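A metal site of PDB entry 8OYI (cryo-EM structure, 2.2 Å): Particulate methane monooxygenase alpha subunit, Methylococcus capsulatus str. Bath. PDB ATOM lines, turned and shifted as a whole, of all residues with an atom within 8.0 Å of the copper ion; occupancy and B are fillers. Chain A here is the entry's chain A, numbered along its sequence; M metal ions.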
ATOM      1  N   MET A  44      11.555 -18.176  -4.609  1.00  0.00           N
ATOM      2  CA  MET A  44      11.206 -19.307  -5.465  1.00  0.00           C
ATOM      3  C   MET A  44       9.701 -19.421  -5.674  1.00  0.00           C
ATOM      4  O   MET A  44       9.257 -19.666  -6.794  1.00  0.00           O
ATOM      5  CB  MET A  44      11.747 -20.605  -4.869  1.00  0.00           C
ATOM      6  CG  MET A  44      13.229 -20.820  -5.085  1.00  0.00           C
ATOM      7  SD  MET A  44      13.923 -21.998  -3.903  1.00  0.00           S
ATOM      8  CE  MET A  44      15.524 -22.302  -4.634  1.00  0.00           C
ATOM      9  N   ARG A  45       8.910 -19.248  -4.624  1.00  0.00           N
ATOM     10  CA  ARG A  45       7.468 -19.415  -4.725  1.00  0.00           C
ATOM     11  C   ARG A  45       6.769 -18.093  -4.404  1.00  0.00           C
ATOM     12  O   ARG A  45       6.147 -17.943  -3.356  1.00  0.00           O
ATOM     13  CB  ARG A  45       7.021 -20.523  -3.760  1.00  0.00           C
ATOM     14  CG  ARG A  45       8.066 -21.586  -3.492  1.00  0.00           C
ATOM     15  CD  ARG A  45       7.941 -22.170  -2.089  1.00  0.00           C
ATOM     16  NE  ARG A  45       6.589 -22.655  -1.808  1.00  0.00           N
ATOM     17  CZ  ARG A  45       6.129 -23.840  -2.189  1.00  0.00           C
ATOM     18  NH1 ARG A  45       6.873 -24.694  -2.869  1.00  0.00           N
ATOM     19  NH2 ARG A  45       4.882 -24.186  -1.869  1.00  0.00           N
ATOM     20  N   THR A  46       6.860 -17.142  -5.319  1.00  0.00           N
ATOM     21  CA  THR A  46       5.881 -16.068  -5.389  1.00  0.00           C
ATOM     22  C   THR A  46       5.378 -15.882  -6.816  1.00  0.00           C
ATOM     23  O   THR A  46       4.194 -16.040  -7.101  1.00  0.00           O
ATOM     24  CB  THR A  46       6.467 -14.761  -4.851  1.00  0.00           C
ATOM     25  OG1 THR A  46       7.852 -14.665  -5.219  1.00  0.00           O
ATOM     26  CG2 THR A  46       6.331 -14.699  -3.345  1.00  0.00           C
ATOM     27  N   ILE A  47       6.314 -15.575  -7.725  1.00  0.00           N
ATOM     28  CA  ILE A  47       6.011 -15.153  -9.081  1.00  0.00           C
ATOM     29  C   ILE A  47       7.167 -15.588  -9.968  1.00  0.00           C
ATOM     30  O   ILE A  47       8.331 -15.289  -9.664  1.00  0.00           O
ATOM     31  CB  ILE A  47       5.796 -13.633  -9.193  1.00  0.00           C
ATOM     32  CG1 ILE A  47       4.413 -13.246  -8.686  1.00  0.00           C
ATOM     33  CG2 ILE A  47       5.998 -13.165 -10.622  1.00  0.00           C
ATOM     34  CD1 ILE A  47       4.193 -11.758  -8.602  1.00  0.00           C
ATOM     35  N   HIS A  48       6.869 -16.299 -11.040  1.00  0.00           N
ATOM     36  CA  HIS A  48       7.886 -16.793 -11.963  1.00  0.00           C
ATOM     37  C   HIS A  48       7.863 -15.957 -13.230  1.00  0.00           C
ATOM     38  O   HIS A  48       6.861 -15.936 -13.957  1.00  0.00           O
ATOM     39  CB  HIS A  48       7.661 -18.269 -12.279  1.00  0.00           C
ATOM     40  CG  HIS A  48       7.590 -19.137 -11.054  1.00  0.00           C
ATOM     41  ND1 HIS A  48       6.703 -20.177 -10.930  1.00  0.00           N
ATOM     42  CD2 HIS A  48       8.302 -19.103  -9.906  1.00  0.00           C
ATOM     43  CE1 HIS A  48       6.872 -20.752  -9.757  1.00  0.00           C
ATOM     44  NE2 HIS A  48       7.834 -20.120  -9.110  1.00  0.00           N
ATOM     45  N   TRP A  49       8.968 -15.269 -13.513  1.00  0.00           N
ATOM     46  CA  TRP A  49       9.108 -14.439 -14.692  1.00  0.00           C
ATOM     47  C   TRP A  49       9.785 -15.239 -15.789  1.00  0.00           C
ATOM     48  O   TRP A  49      10.835 -15.847 -15.575  1.00  0.00           O
ATOM     49  CB  TRP A  49       9.933 -13.183 -14.390  1.00  0.00           C
ATOM     50  CG  TRP A  49       9.517 -12.444 -13.144  1.00  0.00           C
ATOM     51  CD1 TRP A  49       9.852 -12.765 -11.865  1.00  0.00           C
ATOM     52  CD2 TRP A  49       8.719 -11.265 -13.071  1.00  0.00           C
ATOM     53  NE1 TRP A  49       9.294 -11.859 -10.996  1.00  0.00           N
ATOM     54  CE2 TRP A  49       8.593 -10.925 -11.710  1.00  0.00           C
ATOM     55  CE3 TRP A  49       8.088 -10.461 -14.024  1.00  0.00           C
ATOM     56  CZ2 TRP A  49       7.872  -9.821 -11.283  1.00  0.00           C
ATOM     57  CZ3 TRP A  49       7.366  -9.357 -13.596  1.00  0.00           C
ATOM     58  CH2 TRP A  49       7.265  -9.053 -12.229  1.00  0.00           C
ATOM     59  N   TYR A  50       9.189 -15.233 -16.982  1.00  0.00           N
ATOM     60  CA  TYR A  50       9.782 -15.919 -18.125  1.00  0.00           C
ATOM     61  C   TYR A  50       9.330 -15.220 -19.398  1.00  0.00           C
ATOM     62  O   TYR A  50       8.463 -14.346 -19.383  1.00  0.00           O
ATOM     63  CB  TYR A  50       9.413 -17.411 -18.143  1.00  0.00           C
ATOM     64  CG  TYR A  50       7.949 -17.715 -18.368  1.00  0.00           C
ATOM     65  CD1 TYR A  50       7.031 -17.607 -17.328  1.00  0.00           C
ATOM     66  CD2 TYR A  50       7.490 -18.112 -19.616  1.00  0.00           C
ATOM     67  CE1 TYR A  50       5.698 -17.885 -17.530  1.00  0.00           C
ATOM     68  CE2 TYR A  50       6.156 -18.395 -19.826  1.00  0.00           C
ATOM     69  CZ  TYR A  50       5.271 -18.283 -18.773  1.00  0.00           C
ATOM     70  OH  TYR A  50       3.936 -18.566 -18.982  1.00  0.00           O
ATOM     71  N   PHE A  71       4.633 -13.273 -16.419  1.00  0.00           N
ATOM     72  CA  PHE A  71       4.818 -13.722 -15.051  1.00  0.00           C
ATOM     73  C   PHE A  71       3.657 -14.600 -14.647  1.00  0.00           C
ATOM     74  O   PHE A  71       2.507 -14.349 -15.011  1.00  0.00           O
ATOM     75  CB  PHE A  71       4.976 -12.539 -14.071  1.00  0.00           C
ATOM     76  CG  PHE A  71       3.773 -11.646 -13.983  1.00  0.00           C
ATOM     77  CD1 PHE A  71       2.767 -11.904 -13.053  1.00  0.00           C
ATOM     78  CD2 PHE A  71       3.649 -10.545 -14.798  1.00  0.00           C
ATOM     79  CE1 PHE A  71       1.673 -11.081 -12.958  1.00  0.00           C
ATOM     80  CE2 PHE A  71       2.547  -9.712 -14.707  1.00  0.00           C
ATOM     81  CZ  PHE A  71       1.557  -9.988 -13.781  1.00  0.00           C
ATOM     82  N   HIS A  72       3.964 -15.664 -13.904  1.00  0.00           N
ATOM     83  CA  HIS A  72       2.973 -16.608 -13.424  1.00  0.00           C
ATOM     84  C   HIS A  72       2.906 -16.519 -11.904  1.00  0.00           C
ATOM     85  O   HIS A  72       3.930 -16.611 -11.220  1.00  0.00           O
ATOM     86  CB  HIS A  72       3.319 -18.038 -13.853  1.00  0.00           C
ATOM     87  CG  HIS A  72       2.433 -19.083 -13.255  1.00  0.00           C
ATOM     88  ND1 HIS A  72       2.892 -20.033 -12.381  1.00  0.00           N
ATOM     89  CD2 HIS A  72       1.106 -19.312 -13.404  1.00  0.00           C
ATOM     90  CE1 HIS A  72       1.899 -20.817 -12.022  1.00  0.00           C
ATOM     91  NE2 HIS A  72       0.797 -20.398 -12.627  1.00  0.00           N
ATOM     92  N   VAL A  73       1.696 -16.350 -11.378  1.00  0.00           N
ATOM     93  CA  VAL A  73       1.489 -16.299  -9.933  1.00  0.00           C
ATOM     94  C   VAL A  73       1.420 -17.726  -9.415  1.00  0.00           C
ATOM     95  O   VAL A  73       0.538 -18.507  -9.807  1.00  0.00           O
ATOM     96  CB  VAL A  73       0.219 -15.521  -9.588  1.00  0.00           C
ATOM     97  CG1 VAL A  73       0.151 -15.275  -8.090  1.00  0.00           C
ATOM     98  CG2 VAL A  73       0.189 -14.202 -10.341  1.00  0.00           C
ATOM     99  N   PHE A  74       2.359 -18.088  -8.536  1.00  0.00           N
ATOM    100  CA  PHE A  74       2.478 -19.467  -8.074  1.00  0.00           C
ATOM    101  C   PHE A  74       1.269 -19.863  -7.233  1.00  0.00           C
ATOM    102  O   PHE A  74       0.772 -19.079  -6.419  1.00  0.00           O
ATOM    103  CB  PHE A  74       3.757 -19.636  -7.265  1.00  0.00           C
ATOM    104  CG  PHE A  74       3.986 -21.034  -6.794  1.00  0.00           C
ATOM    105  CD1 PHE A  74       3.945 -22.098  -7.675  1.00  0.00           C
ATOM    106  CD2 PHE A  74       4.247 -21.296  -5.463  1.00  0.00           C
ATOM    107  CE1 PHE A  74       4.150 -23.389  -7.247  1.00  0.00           C
ATOM    108  CE2 PHE A  74       4.462 -22.591  -5.022  1.00  0.00           C
ATOM    109  CZ  PHE A  74       4.414 -23.637  -5.914  1.00  0.00           C
ATOM    110  N   GLU A  75       0.788 -21.094  -7.441  1.00  0.00           N
ATOM    111  CA  GLU A  75      -0.368 -21.581  -6.699  1.00  0.00           C
ATOM    112  C   GLU A  75      -0.080 -21.698  -5.215  1.00  0.00           C
ATOM    113  O   GLU A  75      -0.926 -21.375  -4.379  1.00  0.00           O
ATOM    114  CB  GLU A  75      -0.822 -22.935  -7.263  1.00  0.00           C
ATOM    115  CG  GLU A  75      -1.547 -22.834  -8.588  1.00  0.00           C
ATOM    116  CD  GLU A  75      -0.594 -22.793  -9.777  1.00  0.00           C
ATOM    117  OE1 GLU A  75       0.624 -22.788  -9.544  1.00  0.00           O
ATOM    118  OE2 GLU A  75      -1.078 -22.768 -10.925  1.00  0.00           O
ATOM    119  N   GLY A  76       1.116 -22.171  -4.858  1.00  0.00           N
ATOM    120  CA  GLY A  76       1.497 -22.288  -3.459  1.00  0.00           C
ATOM    121  C   GLY A  76       1.984 -20.979  -2.885  1.00  0.00           C
ATOM    122  O   GLY A  76       3.089 -20.908  -2.321  1.00  0.00           O
ATOM    123  N   GLY A 119      -2.309 -18.517  -9.535  1.00  0.00           N
ATOM    124  CA  GLY A 119      -2.339 -19.565 -10.530  1.00  0.00           C
ATOM    125  C   GLY A 119      -2.451 -19.078 -11.954  1.00  0.00           C
ATOM    126  O   GLY A 119      -2.332 -19.893 -12.874  1.00  0.00           O
ATOM    127  N   LYS A 120      -2.693 -17.787 -12.163  1.00  0.00           N
ATOM    128  CA  LYS A 120      -2.856 -17.244 -13.500  1.00  0.00           C
ATOM    129  C   LYS A 120      -1.525 -16.719 -14.039  1.00  0.00           C
ATOM    130  O   LYS A 120      -0.637 -16.308 -13.283  1.00  0.00           O
ATOM    131  CB  LYS A 120      -3.890 -16.125 -13.500  1.00  0.00           C
ATOM    132  CG  LYS A 120      -5.311 -16.583 -13.245  1.00  0.00           C
ATOM    133  CD  LYS A 120      -5.850 -17.353 -14.439  1.00  0.00           C
ATOM    134  CE  LYS A 120      -7.005 -18.255 -14.032  1.00  0.00           C
ATOM    135  NZ  LYS A 120      -7.773 -18.748 -15.209  1.00  0.00           N
ATOM    136  N   THR A 121      -1.392 -16.745 -15.358  1.00  0.00           N
ATOM    137  CA  THR A 121      -0.242 -16.213 -16.055  1.00  0.00           C
ATOM    138  C   THR A 121      -0.649 -14.939 -16.781  1.00  0.00           C
ATOM    139  O   THR A 121      -1.655 -14.940 -17.505  1.00  0.00           O
ATOM    140  CB  THR A 121       0.342 -17.222 -17.047  1.00  0.00           C
ATOM    141  OG1 THR A 121       0.699 -18.422 -16.347  1.00  0.00           O
ATOM    142  CG2 THR A 121       1.574 -16.652 -17.728  1.00  0.00           C
ATOM    143  N   TYR A 318      13.868 -23.116 -14.449  1.00  0.00           N
ATOM    144  CA  TYR A 318      13.878 -21.782 -13.869  1.00  0.00           C
ATOM    145  C   TYR A 318      13.328 -21.892 -12.450  1.00  0.00           C
ATOM    146  O   TYR A 318      12.220 -22.396 -12.255  1.00  0.00           O
ATOM    147  CB  TYR A 318      13.035 -20.816 -14.719  1.00  0.00           C
ATOM    148  CG  TYR A 318      12.658 -19.501 -14.077  1.00  0.00           C
ATOM    149  CD1 TYR A 318      11.574 -19.409 -13.207  1.00  0.00           C
ATOM    150  CD2 TYR A 318      13.378 -18.348 -14.348  1.00  0.00           C
ATOM    151  CE1 TYR A 318      11.228 -18.208 -12.632  1.00  0.00           C
ATOM    152  CE2 TYR A 318      13.031 -17.147 -13.773  1.00  0.00           C
ATOM    153  CZ  TYR A 318      11.952 -17.076 -12.914  1.00  0.00           C
ATOM    154  OH  TYR A 318      11.615 -15.877 -12.340  1.00  0.00           O
ATOM    155  N   THR A 319      14.090 -21.425 -11.464  1.00  0.00           N
ATOM    156  CA  THR A 319      13.698 -21.553 -10.060  1.00  0.00           C
ATOM    157  C   THR A 319      13.411 -20.190  -9.438  1.00  0.00           C
ATOM    158  O   THR A 319      12.289 -19.966  -8.959  1.00  0.00           O
ATOM    159  CB  THR A 319      14.758 -22.330  -9.272  1.00  0.00           C
ATOM    160  OG1 THR A 319      14.492 -22.193  -7.872  1.00  0.00           O
ATOM    161  CG2 THR A 319      16.160 -21.828  -9.590  1.00  0.00           C
ATOM    162  N   ALA A 388       9.985 -24.007  -5.661  1.00  0.00           N
ATOM    163  CA  ALA A 388       9.093 -24.067  -6.808  1.00  0.00           C
ATOM    164  C   ALA A 388       9.854 -23.546  -8.018  1.00  0.00           C
ATOM    165  O   ALA A 388      10.815 -22.783  -7.895  1.00  0.00           O
ATOM    166  CB  ALA A 388       7.815 -23.250  -6.599  1.00  0.00           C
ATOM    167  N   GLY A 389       9.418 -23.965  -9.207  1.00  0.00           N
ATOM    168  CA  GLY A 389      10.097 -23.545 -10.414  1.00  0.00           C
ATOM    169  C   GLY A 389       9.291 -23.896 -11.642  1.00  0.00           C
ATOM    170  O   GLY A 389       8.161 -24.391 -11.559  1.00  0.00           O
ATOM    171  N   LEU A 390       9.883 -23.626 -12.798  1.00  0.00           N
ATOM    172  CA  LEU A 390       9.287 -23.921 -14.082  1.00  0.00           C
ATOM    173  C   LEU A 390      10.238 -24.801 -14.883  1.00  0.00           C
ATOM    174  O   LEU A 390      11.438 -24.513 -14.965  1.00  0.00           O
ATOM    175  CB  LEU A 390       8.976 -22.651 -14.866  1.00  0.00           C
ATOM    176  CG  LEU A 390       8.009 -21.649 -14.243  1.00  0.00           C
ATOM    177  CD1 LEU A 390       7.845 -20.442 -15.158  1.00  0.00           C
ATOM    178  CD2 LEU A 390       6.662 -22.300 -13.985  1.00  0.00           C
ATOM    179  N   VAL A 402       5.540 -25.514 -20.903  1.00  0.00           N
ATOM    180  CA  VAL A 402       5.905 -25.014 -19.579  1.00  0.00           C
ATOM    181  C   VAL A 402       5.138 -25.820 -18.543  1.00  0.00           C
ATOM    182  O   VAL A 402       3.900 -25.841 -18.561  1.00  0.00           O
ATOM    183  CB  VAL A 402       5.603 -23.510 -19.435  1.00  0.00           C
ATOM    184  CG1 VAL A 402       6.145 -22.996 -18.115  1.00  0.00           C
ATOM    185  CG2 VAL A 402       6.185 -22.736 -20.600  1.00  0.00           C
ATOM    186  N   VAL A 403       5.867 -26.467 -17.649  1.00  0.00           N
ATOM    187  CA  VAL A 403       5.259 -27.189 -16.537  1.00  0.00           C
ATOM    188  C   VAL A 403       5.872 -26.665 -15.242  1.00  0.00           C
ATOM    189  O   VAL A 403       7.047 -26.276 -15.189  1.00  0.00           O
ATOM    190  CB  VAL A 403       5.435 -28.720 -16.655  1.00  0.00           C
ATOM    191  CG1 VAL A 403       5.149 -29.186 -18.073  1.00  0.00           C
ATOM    192  CG2 VAL A 403       6.824 -29.155 -16.212  1.00  0.00           C
ATOM    193  N   GLN A 404       5.046 -26.607 -14.204  1.00  0.00           N
ATOM    194  CA  GLN A 404       5.446 -26.072 -12.912  1.00  0.00           C
ATOM    195  C   GLN A 404       5.652 -27.211 -11.930  1.00  0.00           C
ATOM    196  O   GLN A 404       4.844 -28.136 -11.857  1.00  0.00           O
ATOM    197  CB  GLN A 404       4.391 -25.093 -12.388  1.00  0.00           C
ATOM    198  CG  GLN A 404       4.689 -24.540 -11.020  1.00  0.00           C
ATOM    199  CD  GLN A 404       3.856 -23.320 -10.707  1.00  0.00           C
ATOM    200  OE1 GLN A 404       4.335 -22.187 -10.791  1.00  0.00           O
ATOM    201  NE2 GLN A 404       2.599 -23.540 -10.335  1.00  0.00           N
ATOM    202  N   ILE A 405       6.740 -27.132 -11.170  1.00  0.00           N
ATOM    203  CA  ILE A 405       7.077 -28.141 -10.175  1.00  0.00           C
ATOM    204  C   ILE A 405       7.307 -27.459  -8.829  1.00  0.00           C
ATOM    205  O   ILE A 405       7.819 -26.343  -8.774  1.00  0.00           O
ATOM    206  CB  ILE A 405       8.311 -28.959 -10.582  1.00  0.00           C
ATOM    207  CG1 ILE A 405       9.493 -28.036 -10.887  1.00  0.00           C
ATOM    208  CG2 ILE A 405       7.995 -29.844 -11.778  1.00  0.00           C
ATOM    209  CD1 ILE A 405      10.818 -28.746 -10.957  1.00  0.00           C
HETATM  210 CU    CU M   1       4.690 -19.891 -11.360  1.00  0.00          CU
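NE2 of His 72 lies within hydrogen-bond range of OE2 of Glu 75 (3.5 Å). NE2 of His 72 lies within hydrogen-bond range of O of Gly 119 (3.2 Å). The backbone carbonyl oxygen (O) of Met 44 is in hydrogen-bond range of a ring nitrogen (NE2) of His 48, 2.8 Å away. N of Phe 74 sits at hydrogen-bond distance from O of Thr 46 (3.1 Å).
Phe 74 touches the copper ion. Four residues have an atom within 4 Å of the copper ion: His 48, His 72, Phe 74 and Gln 404. The nearest printed residue that does not touch the copper ion is Leu 390 (4.1 Å).
The copper ion is bound by a ring nitrogen (ND1) of His 72 (2.1 Å), a ring nitrogen (ND1) of His 48 (2.1 Å) and the side-chain amide oxygen (OE1) of Gln 404 (2.4 Å). The copper ion has three donor atoms within binding distance.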
